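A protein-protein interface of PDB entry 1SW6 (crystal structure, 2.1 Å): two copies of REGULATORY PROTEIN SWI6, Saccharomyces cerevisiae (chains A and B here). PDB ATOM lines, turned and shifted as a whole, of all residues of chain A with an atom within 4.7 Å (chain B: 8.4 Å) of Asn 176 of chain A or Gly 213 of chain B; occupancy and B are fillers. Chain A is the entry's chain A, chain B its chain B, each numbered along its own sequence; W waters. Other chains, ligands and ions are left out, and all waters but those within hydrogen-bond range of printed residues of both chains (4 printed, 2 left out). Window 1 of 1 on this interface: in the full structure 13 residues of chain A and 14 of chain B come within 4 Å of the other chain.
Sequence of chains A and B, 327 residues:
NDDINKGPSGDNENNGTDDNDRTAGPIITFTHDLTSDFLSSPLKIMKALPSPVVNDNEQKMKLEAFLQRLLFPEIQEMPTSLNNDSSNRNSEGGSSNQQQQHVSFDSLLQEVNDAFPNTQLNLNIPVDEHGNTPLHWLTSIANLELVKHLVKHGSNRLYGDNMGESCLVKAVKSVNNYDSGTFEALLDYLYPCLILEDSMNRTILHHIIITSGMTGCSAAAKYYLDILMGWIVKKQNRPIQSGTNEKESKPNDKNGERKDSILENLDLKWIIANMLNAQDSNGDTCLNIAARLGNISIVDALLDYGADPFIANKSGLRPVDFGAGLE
O of Gly 213 of chain B touches CD1 of Ile 141 of chain A, 3.0 Å away. Ile 141 of chain A touches Met 214 of chain B (CD1 to CA, 3.3 Å). SG of Cys 217 of chain B touches CG1 of Val 175 of chain A, at 3.6 Å. Val 175 of chain A touches Asn 295 of chain B. O of Asn 176 of chain A touches O of Gly 294 of chain B (3.7 Å). Asn 295 of chain B touches Asn 176 of chain A. Gly 294 of chain B touches Asp 179 of chain A. OD2 of Asp 179 of chain A touches C of Asn 295 of chain B (3.8 Å). O of Gly 294 of chain B touches OG of Ser 180 of chain A, 3.5 Å away.
O of Ser 140 of chain A sits at hydrogen-bond distance from OG of Ser 174 of chain A (3.0 Å). O of Cys 217 of chain B sits at hydrogen-bond distance from NZ of Lys 222 of chain B, at 3.3 Å. The side-chain amide oxygen of Asn 295 of chain B lies within hydrogen-bond range of the side-chain hydroxyl of Ser 297 of chain B (2.4 Å). The backbone NH (N) of Ile 298 of chain B lies within hydrogen-bond range of the side-chain amide oxygen (OD1) of Asn 295 of chain B (3.4 Å). The backbone carbonyl oxygen (O) of Asn 176 of chain A lies within hydrogen-bond range of the side-chain hydroxyl (OG) of Ser 180 of chain A (2.9 Å).
Water W2 lies within hydrogen-bond range of OD2 of Asp 179 of chain A (2.5 Å), N of Ser 297 of chain B (3.1 Å) and OD1 of Asn 295 of chain B (3.3 Å). Water W3 bridges O of Arg 292 of chain B (2.8 Å) and O of Ile 141 of chain A (2.9 Å). Water W1 bridges the side-chain hydroxyl (OG) of Ser 180 of chain A (2.9 Å) and the backbone carbonyl oxygen (O) of Gly 294 of chain B (2.9 Å). Water W4 bridges N of Val 175 of chain A and SG of Cys 217 of chain B.
Of chain B, only Gly 213 (3.3 Å), Leu 293 (2.7 Å), Gly 294 (3.7 Å) and Asn 295 (3.9 Å) come within 4 Å of Asn 176 of chain A. Of chain A, only Ile 141 (3.0 Å) and Asn 176 (3.3 Å) come within 4 Å of Gly 213 of chain B. Of the printed residues of chain A, Leu 293 of chain B touches Ile 141 (3.1 Å) and Asn 176 (2.7 Å). Printed residues of chain A within 4 Å of Asn 295 of chain B: Val 175, Asn 176 and Asp 179. Of the printed residues of chain A, Ile 296 of chain B touches Asp 179. The nearest residue of chain B that does not touch Asn 176 of chain A is Thr 215 of chain B (4.9 Å). The nearest printed residue of chain A that does not touch Gly 213 of chain B is Ser 140 of chain A (4.7 Å). The nearest printed residue of chain A that does not touch Ile 296 of chain B is Ser 180 of chain A (5.3 Å).
ND2 of Asn 176 of chain A is in hydrogen-bond range of O of Gly 213 of chain B (3.3 Å). The side-chain amide nitrogen (ND2) of Asn 176 of chain A lies within hydrogen-bond range of the backbone carbonyl oxygen (O) of Leu 293 of chain B (2.7 Å). The backbone NH (N) of Ile 296 of chain B is in hydrogen-bond range of the side-chain carboxylate (OD2) of Asp 179 of chain A (3.0 Å). O of Met 214 of chain B is in hydrogen-bond range of OG of Ser 140 of chain A, at 3.4 Å. O of Leu 293 of chain B sits close to O of Ile 141 of chain A, 3.1 Å away.
Printed residues of chain B that touch a printed residue of chain A: Gly 213, Met 214, Cys 217, Leu 293, Gly 294, Asn 295 and Ile 296. Of the 11 printed residues of chain A, 6 touch a printed residue of chain B. Printed residues of chain A that touch a printed residue of chain B: Ser 140, Ile 141, Val 175, Asn 176, Asp 179 and Ser 180. Hydrophobic or aromatic side chains of chain A that line the printed part of chain B: Ile 141 and Val 175. Among the printed residues, no Asp or Glu carboxylate lies within 4 Å of a Lys or Arg side-chain nitrogen of the other chain.
No position is printed for both chains.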
ATOM      1  N   SER A 140      -0.006   1.612  15.133  1.00  0.00           N
ATOM      2  CA  SER A 140       0.357   3.016  15.284  1.00  0.00           C
ATOM      3  C   SER A 140      -0.817   3.915  14.900  1.00  0.00           C
ATOM      4  O   SER A 140      -0.943   5.040  15.365  1.00  0.00           O
ATOM      5  CB  SER A 140       1.555   3.335  14.387  1.00  0.00           C
ATOM      6  OG  SER A 140       2.046   4.640  14.637  1.00  0.00           O
ATOM      7  N   ILE A 141      -1.682   3.374  14.060  1.00  0.00           N
ATOM      8  CA  ILE A 141      -2.828   4.086  13.531  1.00  0.00           C
ATOM      9  C   ILE A 141      -4.131   3.740  14.241  1.00  0.00           C
ATOM     10  O   ILE A 141      -5.210   4.143  13.815  1.00  0.00           O
ATOM     11  CB  ILE A 141      -2.905   3.785  12.003  1.00  0.00           C
ATOM     12  CG1 ILE A 141      -2.830   5.086  11.239  1.00  0.00           C
ATOM     13  CG2 ILE A 141      -4.094   2.913  11.659  1.00  0.00           C
ATOM     14  CD1 ILE A 141      -1.507   5.759  11.399  1.00  0.00           C
ATOM     15  N   ALA A 142      -4.018   2.992  15.331  1.00  0.00           N
ATOM     16  CA  ALA A 142      -5.169   2.575  16.119  1.00  0.00           C
ATOM     17  C   ALA A 142      -6.233   1.819  15.327  1.00  0.00           C
ATOM     18  O   ALA A 142      -7.417   1.852  15.688  1.00  0.00           O
ATOM     19  CB  ALA A 142      -5.802   3.778  16.817  1.00  0.00           C
ATOM     20  N   SER A 174       2.209   7.247  19.794  1.00  0.00           N
ATOM     21  CA  SER A 174       1.321   8.108  19.000  1.00  0.00           C
ATOM     22  C   SER A 174       0.033   8.333  19.808  1.00  0.00           C
ATOM     23  O   SER A 174      -0.295   7.536  20.699  1.00  0.00           O
ATOM     24  CB  SER A 174       0.994   7.465  17.649  1.00  0.00           C
ATOM     25  OG  SER A 174       0.114   6.372  17.798  1.00  0.00           O
ATOM     26  N   VAL A 175      -0.686   9.417  19.516  1.00  0.00           N
ATOM     27  CA  VAL A 175      -1.908   9.717  20.260  1.00  0.00           C
ATOM     28  C   VAL A 175      -3.114   9.025  19.677  1.00  0.00           C
ATOM     29  O   VAL A 175      -4.208   9.101  20.233  1.00  0.00           O
ATOM     30  CB  VAL A 175      -2.231  11.227  20.287  1.00  0.00           C
ATOM     31  CG1 VAL A 175      -1.035  12.010  20.786  1.00  0.00           C
ATOM     32  CG2 VAL A 175      -2.678  11.690  18.909  1.00  0.00           C
ATOM     33  N   ASN A 176      -2.908   8.348  18.559  1.00  0.00           N
ATOM     34  CA  ASN A 176      -3.983   7.661  17.857  1.00  0.00           C
ATOM     35  C   ASN A 176      -4.874   6.732  18.676  1.00  0.00           C
ATOM     36  O   ASN A 176      -6.094   6.748  18.516  1.00  0.00           O
ATOM     37  CB  ASN A 176      -3.395   6.902  16.669  1.00  0.00           C
ATOM     38  CG  ASN A 176      -2.793   7.833  15.638  1.00  0.00           C
ATOM     39  OD1 ASN A 176      -1.954   8.676  15.972  1.00  0.00           O
ATOM     40  ND2 ASN A 176      -3.216   7.692  14.379  1.00  0.00           N
ATOM     41  N   ASN A 177      -4.281   5.913  19.542  1.00  0.00           N
ATOM     42  CA  ASN A 177      -5.076   4.985  20.335  1.00  0.00           C
ATOM     43  C   ASN A 177      -5.846   5.661  21.467  1.00  0.00           C
ATOM     44  O   ASN A 177      -6.865   5.157  21.919  1.00  0.00           O
ATOM     45  CB  ASN A 177      -4.190   3.857  20.842  1.00  0.00           C
ATOM     46  CG  ASN A 177      -3.969   2.788  19.778  1.00  0.00           C
ATOM     47  OD1 ASN A 177      -4.787   1.901  19.625  1.00  0.00           O
ATOM     48  ND2 ASN A 177      -2.882   2.894  19.027  1.00  0.00           N
ATOM     49  N   TYR A 178      -5.365   6.816  21.907  1.00  0.00           N
ATOM     50  CA  TYR A 178      -6.052   7.572  22.949  1.00  0.00           C
ATOM     51  C   TYR A 178      -7.241   8.298  22.292  1.00  0.00           C
ATOM     52  O   TYR A 178      -8.380   8.188  22.734  1.00  0.00           O
ATOM     53  CB  TYR A 178      -5.077   8.569  23.577  1.00  0.00           C
ATOM     54  CG  TYR A 178      -5.711   9.676  24.393  1.00  0.00           C
ATOM     55  CD1 TYR A 178      -6.483   9.397  25.516  1.00  0.00           C
ATOM     56  CD2 TYR A 178      -5.504  11.004  24.059  1.00  0.00           C
ATOM     57  CE1 TYR A 178      -7.031  10.424  26.286  1.00  0.00           C
ATOM     58  CE2 TYR A 178      -6.042  12.033  24.819  1.00  0.00           C
ATOM     59  CZ  TYR A 178      -6.803  11.738  25.927  1.00  0.00           C
ATOM     60  OH  TYR A 178      -7.335  12.768  26.662  1.00  0.00           O
ATOM     61  N   ASP A 179      -6.972   9.021  21.214  1.00  0.00           N
ATOM     62  CA  ASP A 179      -8.027   9.743  20.513  1.00  0.00           C
ATOM     63  C   ASP A 179      -9.142   8.807  20.084  1.00  0.00           C
ATOM     64  O   ASP A 179     -10.319   9.161  20.156  1.00  0.00           O
ATOM     65  CB  ASP A 179      -7.466  10.452  19.279  1.00  0.00           C
ATOM     66  CG  ASP A 179      -6.589  11.640  19.637  1.00  0.00           C
ATOM     67  OD1 ASP A 179      -6.475  11.962  20.839  1.00  0.00           O
ATOM     68  OD2 ASP A 179      -6.015  12.257  18.715  1.00  0.00           O
ATOM     69  N   SER A 180      -8.769   7.605  19.657  1.00  0.00           N
ATOM     70  CA  SER A 180      -9.744   6.627  19.194  1.00  0.00           C
ATOM     71  C   SER A 180     -10.321   5.758  20.307  1.00  0.00           C
ATOM     72  O   SER A 180     -11.246   4.989  20.071  1.00  0.00           O
ATOM     73  CB  SER A 180      -9.119   5.731  18.120  1.00  0.00           C
ATOM     74  OG  SER A 180      -8.567   6.509  17.072  1.00  0.00           O
ATOM     75  N   TYR A 224      -2.670   6.177  28.712  1.00  0.00           N
ATOM     76  CA  TYR A 224      -2.058   4.876  28.455  1.00  0.00           C
ATOM     77  C   TYR A 224      -1.603   4.205  29.753  1.00  0.00           C
ATOM     78  O   TYR A 224      -1.870   3.017  29.986  1.00  0.00           O
ATOM     79  CB  TYR A 224      -0.871   5.040  27.490  1.00  0.00           C
ATOM     80  CG  TYR A 224      -1.273   5.432  26.076  1.00  0.00           C
ATOM     81  CD1 TYR A 224      -0.418   6.177  25.277  1.00  0.00           C
ATOM     82  CD2 TYR A 224      -2.508   5.038  25.537  1.00  0.00           C
ATOM     83  CE1 TYR A 224      -0.771   6.536  23.960  1.00  0.00           C
ATOM     84  CE2 TYR A 224      -2.879   5.392  24.223  1.00  0.00           C
ATOM     85  CZ  TYR A 224      -2.003   6.144  23.446  1.00  0.00           C
ATOM     86  OH  TYR A 224      -2.358   6.532  22.172  1.00  0.00           O
ATOM     87  N   HIS B 206      -1.182  16.001   1.120  1.00  0.00           N
ATOM     88  CA  HIS B 206      -1.511  14.584   1.289  1.00  0.00           C
ATOM     89  C   HIS B 206      -0.362  13.887   2.021  1.00  0.00           C
ATOM     90  O   HIS B 206      -0.591  13.131   2.966  1.00  0.00           O
ATOM     91  CB  HIS B 206      -1.722  13.880  -0.061  1.00  0.00           C
ATOM     92  CG  HIS B 206      -3.007  14.231  -0.746  1.00  0.00           C
ATOM     93  ND1 HIS B 206      -3.083  15.173  -1.751  1.00  0.00           N
ATOM     94  CD2 HIS B 206      -4.260  13.732  -0.603  1.00  0.00           C
ATOM     95  CE1 HIS B 206      -4.325  15.233  -2.203  1.00  0.00           C
ATOM     96  NE2 HIS B 206      -5.060  14.368  -1.525  1.00  0.00           N
ATOM     97  N   HIS B 207       0.871  14.135   1.578  1.00  0.00           N
ATOM     98  CA  HIS B 207       2.036  13.518   2.202  1.00  0.00           C
ATOM     99  C   HIS B 207       2.259  13.958   3.649  1.00  0.00           C
ATOM    100  O   HIS B 207       2.592  13.131   4.492  1.00  0.00           O
ATOM    101  CB  HIS B 207       3.297  13.774   1.365  1.00  0.00           C
ATOM    102  CG  HIS B 207       3.348  12.958   0.111  1.00  0.00           C
ATOM    103  ND1 HIS B 207       2.996  13.464  -1.125  1.00  0.00           N
ATOM    104  CD2 HIS B 207       3.615  11.645  -0.082  1.00  0.00           C
ATOM    105  CE1 HIS B 207       3.037  12.495  -2.022  1.00  0.00           C
ATOM    106  NE2 HIS B 207       3.408  11.381  -1.416  1.00  0.00           N
ATOM    107  N   ILE B 208       2.088  15.248   3.941  1.00  0.00           N
ATOM    108  CA  ILE B 208       2.243  15.723   5.313  1.00  0.00           C
ATOM    109  C   ILE B 208       1.192  15.036   6.202  1.00  0.00           C
ATOM    110  O   ILE B 208       1.495  14.548   7.296  1.00  0.00           O
ATOM    111  CB  ILE B 208       2.070  17.262   5.396  1.00  0.00           C
ATOM    112  CG1 ILE B 208       3.274  17.953   4.752  1.00  0.00           C
ATOM    113  CG2 ILE B 208       1.896  17.691   6.843  1.00  0.00           C
ATOM    114  CD1 ILE B 208       3.072  19.433   4.509  1.00  0.00           C
ATOM    115  N   ILE B 209      -0.045  14.979   5.720  1.00  0.00           N
ATOM    116  CA  ILE B 209      -1.093  14.340   6.495  1.00  0.00           C
ATOM    117  C   ILE B 209      -0.810  12.853   6.655  1.00  0.00           C
ATOM    118  O   ILE B 209      -0.935  12.308   7.748  1.00  0.00           O
ATOM    119  CB  ILE B 209      -2.487  14.572   5.849  1.00  0.00           C
ATOM    120  CG1 ILE B 209      -3.100  15.865   6.403  1.00  0.00           C
ATOM    121  CG2 ILE B 209      -3.424  13.408   6.164  1.00  0.00           C
ATOM    122  CD1 ILE B 209      -2.189  17.061   6.355  1.00  0.00           C
ATOM    123  N   ILE B 210      -0.406  12.195   5.575  1.00  0.00           N
ATOM    124  CA  ILE B 210      -0.121  10.768   5.665  1.00  0.00           C
ATOM    125  C   ILE B 210       1.013  10.497   6.639  1.00  0.00           C
ATOM    126  O   ILE B 210       0.885   9.657   7.537  1.00  0.00           O
ATOM    127  CB  ILE B 210       0.250  10.168   4.277  1.00  0.00           C
ATOM    128  CG1 ILE B 210      -0.994  10.139   3.375  1.00  0.00           C
ATOM    129  CG2 ILE B 210       0.814   8.768   4.453  1.00  0.00           C
ATOM    130  CD1 ILE B 210      -0.691   9.830   1.896  1.00  0.00           C
ATOM    131  N   THR B 211       2.119  11.222   6.472  1.00  0.00           N
ATOM    132  CA  THR B 211       3.280  11.021   7.327  1.00  0.00           C
ATOM    133  C   THR B 211       3.005  11.337   8.799  1.00  0.00           C
ATOM    134  O   THR B 211       3.347  10.547   9.676  1.00  0.00           O
ATOM    135  CB  THR B 211       4.464  11.869   6.841  1.00  0.00           C
ATOM    136  OG1 THR B 211       4.820  11.464   5.515  1.00  0.00           O
ATOM    137  CG2 THR B 211       5.668  11.695   7.766  1.00  0.00           C
ATOM    138  N   SER B 212       2.383  12.482   9.077  1.00  0.00           N
ATOM    139  CA  SER B 212       2.109  12.840  10.462  1.00  0.00           C
ATOM    140  C   SER B 212       1.090  11.900  11.093  1.00  0.00           C
ATOM    141  O   SER B 212       1.206  11.553  12.261  1.00  0.00           O
ATOM    142  CB  SER B 212       1.621  14.292  10.564  1.00  0.00           C
ATOM    143  OG  SER B 212       0.380  14.463   9.888  1.00  0.00           O
ATOM    144  N   GLY B 213       0.086  11.483  10.331  1.00  0.00           N
ATOM    145  CA  GLY B 213      -0.913  10.589  10.895  1.00  0.00           C
ATOM    146  C   GLY B 213      -0.381   9.211  11.264  1.00  0.00           C
ATOM    147  O   GLY B 213      -0.876   8.567  12.192  1.00  0.00           O
ATOM    148  N   MET B 214       0.639   8.760  10.540  1.00  0.00           N
ATOM    149  CA  MET B 214       1.223   7.445  10.780  1.00  0.00           C
ATOM    150  C   MET B 214       2.505   7.454  11.583  1.00  0.00           C
ATOM    151  O   MET B 214       3.064   6.405  11.853  1.00  0.00           O
ATOM    152  CB  MET B 214       1.483   6.741   9.462  1.00  0.00           C
ATOM    153  CG  MET B 214       0.230   6.534   8.659  1.00  0.00           C
ATOM    154  SD  MET B 214       0.615   5.646   7.173  1.00  0.00           S
ATOM    155  CE  MET B 214       0.793   3.959   7.873  1.00  0.00           C
ATOM    156  N   THR B 215       2.994   8.631  11.948  1.00  0.00           N
ATOM    157  CA  THR B 215       4.206   8.687  12.751  1.00  0.00           C
ATOM    158  C   THR B 215       3.797   9.084  14.167  1.00  0.00           C
ATOM    159  O   THR B 215       2.640   9.417  14.420  1.00  0.00           O
ATOM    160  CB  THR B 215       5.213   9.705  12.205  1.00  0.00           C
ATOM    161  OG1 THR B 215       5.356   9.530  10.792  1.00  0.00           O
ATOM    162  CG2 THR B 215       6.566   9.472  12.838  1.00  0.00           C
ATOM    163  N   GLY B 216       4.745   9.062  15.088  1.00  0.00           N
ATOM    164  CA  GLY B 216       4.411   9.394  16.458  1.00  0.00           C
ATOM    165  C   GLY B 216       4.588  10.821  16.933  1.00  0.00           C
ATOM    166  O   GLY B 216       4.694  11.769  16.153  1.00  0.00           O
ATOM    167  N   CYS B 217       4.610  10.941  18.256  1.00  0.00           N
ATOM    168  CA  CYS B 217       4.761  12.197  18.962  1.00  0.00           C
ATOM    169  C   CYS B 217       6.182  12.733  18.896  1.00  0.00           C
ATOM    170  O   CYS B 217       6.405  13.932  19.060  1.00  0.00           O
ATOM    171  CB  CYS B 217       4.356  11.992  20.422  1.00  0.00           C
ATOM    172  SG  CYS B 217       2.561  11.774  20.664  1.00  0.00           S
ATOM    173  N   ALA B 221       7.215  15.777  11.878  1.00  0.00           N
ATOM    174  CA  ALA B 221       6.109  15.884  10.911  1.00  0.00           C
ATOM    175  C   ALA B 221       4.819  16.432  11.516  1.00  0.00           C
ATOM    176  O   ALA B 221       3.983  16.996  10.812  1.00  0.00           O
ATOM    177  CB  ALA B 221       5.833  14.532  10.273  1.00  0.00           C
ATOM    178  N   LYS B 222       4.649  16.258  12.820  1.00  0.00           N
ATOM    179  CA  LYS B 222       3.457  16.756  13.502  1.00  0.00           C
ATOM    180  C   LYS B 222       3.347  18.282  13.384  1.00  0.00           C
ATOM    181  O   LYS B 222       2.287  18.848  13.629  1.00  0.00           O
ATOM    182  CB  LYS B 222       3.502  16.375  14.991  1.00  0.00           C
ATOM    183  CG  LYS B 222       4.692  16.999  15.730  1.00  0.00           C
ATOM    184  CD  LYS B 222       4.937  16.386  17.113  1.00  0.00           C
ATOM    185  CE  LYS B 222       4.022  16.975  18.172  1.00  0.00           C
ATOM    186  NZ  LYS B 222       4.344  16.441  19.529  1.00  0.00           N
ATOM    187  N   ILE B 289      -8.231  11.269   4.365  1.00  0.00           N
ATOM    188  CA  ILE B 289      -7.172  10.388   4.842  1.00  0.00           C
ATOM    189  C   ILE B 289      -6.966  10.587   6.349  1.00  0.00           C
ATOM    190  O   ILE B 289      -6.829   9.628   7.101  1.00  0.00           O
ATOM    191  CB  ILE B 289      -5.846  10.674   4.102  1.00  0.00           C
ATOM    192  CG1 ILE B 289      -6.037  10.434   2.605  1.00  0.00           C
ATOM    193  CG2 ILE B 289      -4.722   9.780   4.655  1.00  0.00           C
ATOM    194  CD1 ILE B 289      -4.813  10.770   1.772  1.00  0.00           C
ATOM    195  N   ALA B 290      -6.958  11.838   6.788  1.00  0.00           N
ATOM    196  CA  ALA B 290      -6.782  12.133   8.201  1.00  0.00           C
ATOM    197  C   ALA B 290      -7.926  11.558   9.040  1.00  0.00           C
ATOM    198  O   ALA B 290      -7.727  11.149  10.191  1.00  0.00           O
ATOM    199  CB  ALA B 290      -6.696  13.642   8.407  1.00  0.00           C
ATOM    200  N   ARG B 292      -9.353   8.852   8.625  1.00  0.00           N
ATOM    201  CA  ARG B 292      -9.187   7.418   8.778  1.00  0.00           C
ATOM    202  C   ARG B 292      -7.956   7.037   9.605  1.00  0.00           C
ATOM    203  O   ARG B 292      -7.904   5.946  10.163  1.00  0.00           O
ATOM    204  CB  ARG B 292      -9.134   6.747   7.401  1.00  0.00           C
ATOM    205  CG  ARG B 292     -10.365   7.035   6.531  1.00  0.00           C
ATOM    206  CD  ARG B 292     -10.492   6.044   5.370  1.00  0.00           C
ATOM    207  NE  ARG B 292      -9.352   6.081   4.458  1.00  0.00           N
ATOM    208  CZ  ARG B 292      -9.228   6.930   3.436  1.00  0.00           C
ATOM    209  NH1 ARG B 292     -10.178   7.822   3.182  1.00  0.00           N
ATOM    210  NH2 ARG B 292      -8.146   6.887   2.662  1.00  0.00           N
ATOM    211  N   LEU B 293      -6.971   7.928   9.703  1.00  0.00           N
ATOM    212  CA  LEU B 293      -5.775   7.608  10.474  1.00  0.00           C
ATOM    213  C   LEU B 293      -6.016   7.659  11.991  1.00  0.00           C
ATOM    214  O   LEU B 293      -5.309   7.016  12.762  1.00  0.00           O
ATOM    215  CB  LEU B 293      -4.620   8.517  10.055  1.00  0.00           C
ATOM    216  CG  LEU B 293      -4.225   8.400   8.571  1.00  0.00           C
ATOM    217  CD1 LEU B 293      -3.033   9.301   8.269  1.00  0.00           C
ATOM    218  CD2 LEU B 293      -3.882   6.962   8.235  1.00  0.00           C
ATOM    219  N   GLY B 294      -7.014   8.413  12.428  1.00  0.00           N
ATOM    220  CA  GLY B 294      -7.308   8.449  13.852  1.00  0.00           C
ATOM    221  C   GLY B 294      -6.618   9.462  14.761  1.00  0.00           C
ATOM    222  O   GLY B 294      -6.693   9.319  15.983  1.00  0.00           O
ATOM    223  N   ASN B 295      -5.925  10.454  14.197  1.00  0.00           N
ATOM    224  CA  ASN B 295      -5.292  11.491  15.024  1.00  0.00           C
ATOM    225  C   ASN B 295      -6.275  12.664  14.911  1.00  0.00           C
ATOM    226  O   ASN B 295      -6.365  13.302  13.865  1.00  0.00           O
ATOM    227  CB  ASN B 295      -3.913  11.877  14.474  1.00  0.00           C
ATOM    228  CG  ASN B 295      -3.238  12.977  15.282  1.00  0.00           C
ATOM    229  OD1 ASN B 295      -3.901  13.875  15.801  1.00  0.00           O
ATOM    230  ND2 ASN B 295      -1.906  12.919  15.380  1.00  0.00           N
ATOM    231  N   ILE B 296      -7.036  12.910  15.977  1.00  0.00           N
ATOM    232  CA  ILE B 296      -8.035  13.983  15.996  1.00  0.00           C
ATOM    233  C   ILE B 296      -7.460  15.371  15.747  1.00  0.00           C
ATOM    234  O   ILE B 296      -8.073  16.187  15.056  1.00  0.00           O
ATOM    235  CB  ILE B 296      -8.790  14.031  17.349  1.00  0.00           C
ATOM    236  CG1 ILE B 296      -9.547  12.727  17.577  1.00  0.00           C
ATOM    237  CG2 ILE B 296      -9.774  15.196  17.360  1.00  0.00           C
ATOM    238  CD1 ILE B 296     -10.242  12.659  18.946  1.00  0.00           C
ATOM    239  N   SER B 297      -6.286  15.655  16.306  1.00  0.00           N
ATOM    240  CA  SER B 297      -5.698  16.976  16.120  1.00  0.00           C
ATOM    241  C   SER B 297      -5.447  17.316  14.648  1.00  0.00           C
ATOM    242  O   SER B 297      -5.519  18.485  14.268  1.00  0.00           O
ATOM    243  CB  SER B 297      -4.396  17.103  16.925  1.00  0.00           C
ATOM    244  OG  SER B 297      -3.439  16.116  16.560  1.00  0.00           O
ATOM    245  N   ILE B 298      -5.156  16.302  13.828  1.00  0.00           N
ATOM    246  CA  ILE B 298      -4.885  16.508  12.401  1.00  0.00           C
ATOM    247  C   ILE B 298      -6.204  16.850  11.709  1.00  0.00           C
ATOM    248  O   ILE B 298      -6.275  17.779  10.903  1.00  0.00           O
ATOM    249  CB  ILE B 298      -4.260  15.237  11.755  1.00  0.00           C
ATOM    250  CG1 ILE B 298      -2.929  14.894  12.435  1.00  0.00           C
ATOM    251  CG2 ILE B 298      -4.007  15.464  10.270  1.00  0.00           C
ATOM    252  CD1 ILE B 298      -2.244  13.639  11.851  1.00  0.00           C
HETATM  253  O   HOH W   1      -9.613   9.149  16.314  1.00  0.00           O
HETATM  254  O   HOH W   2      -4.900  14.534  18.866  1.00  0.00           O
HETATM  255  O   HOH W   3      -7.200   3.758  11.696  1.00  0.00           O
HETATM  256  O   HOH W   4       1.087  11.169  17.500  1.00  0.00           O
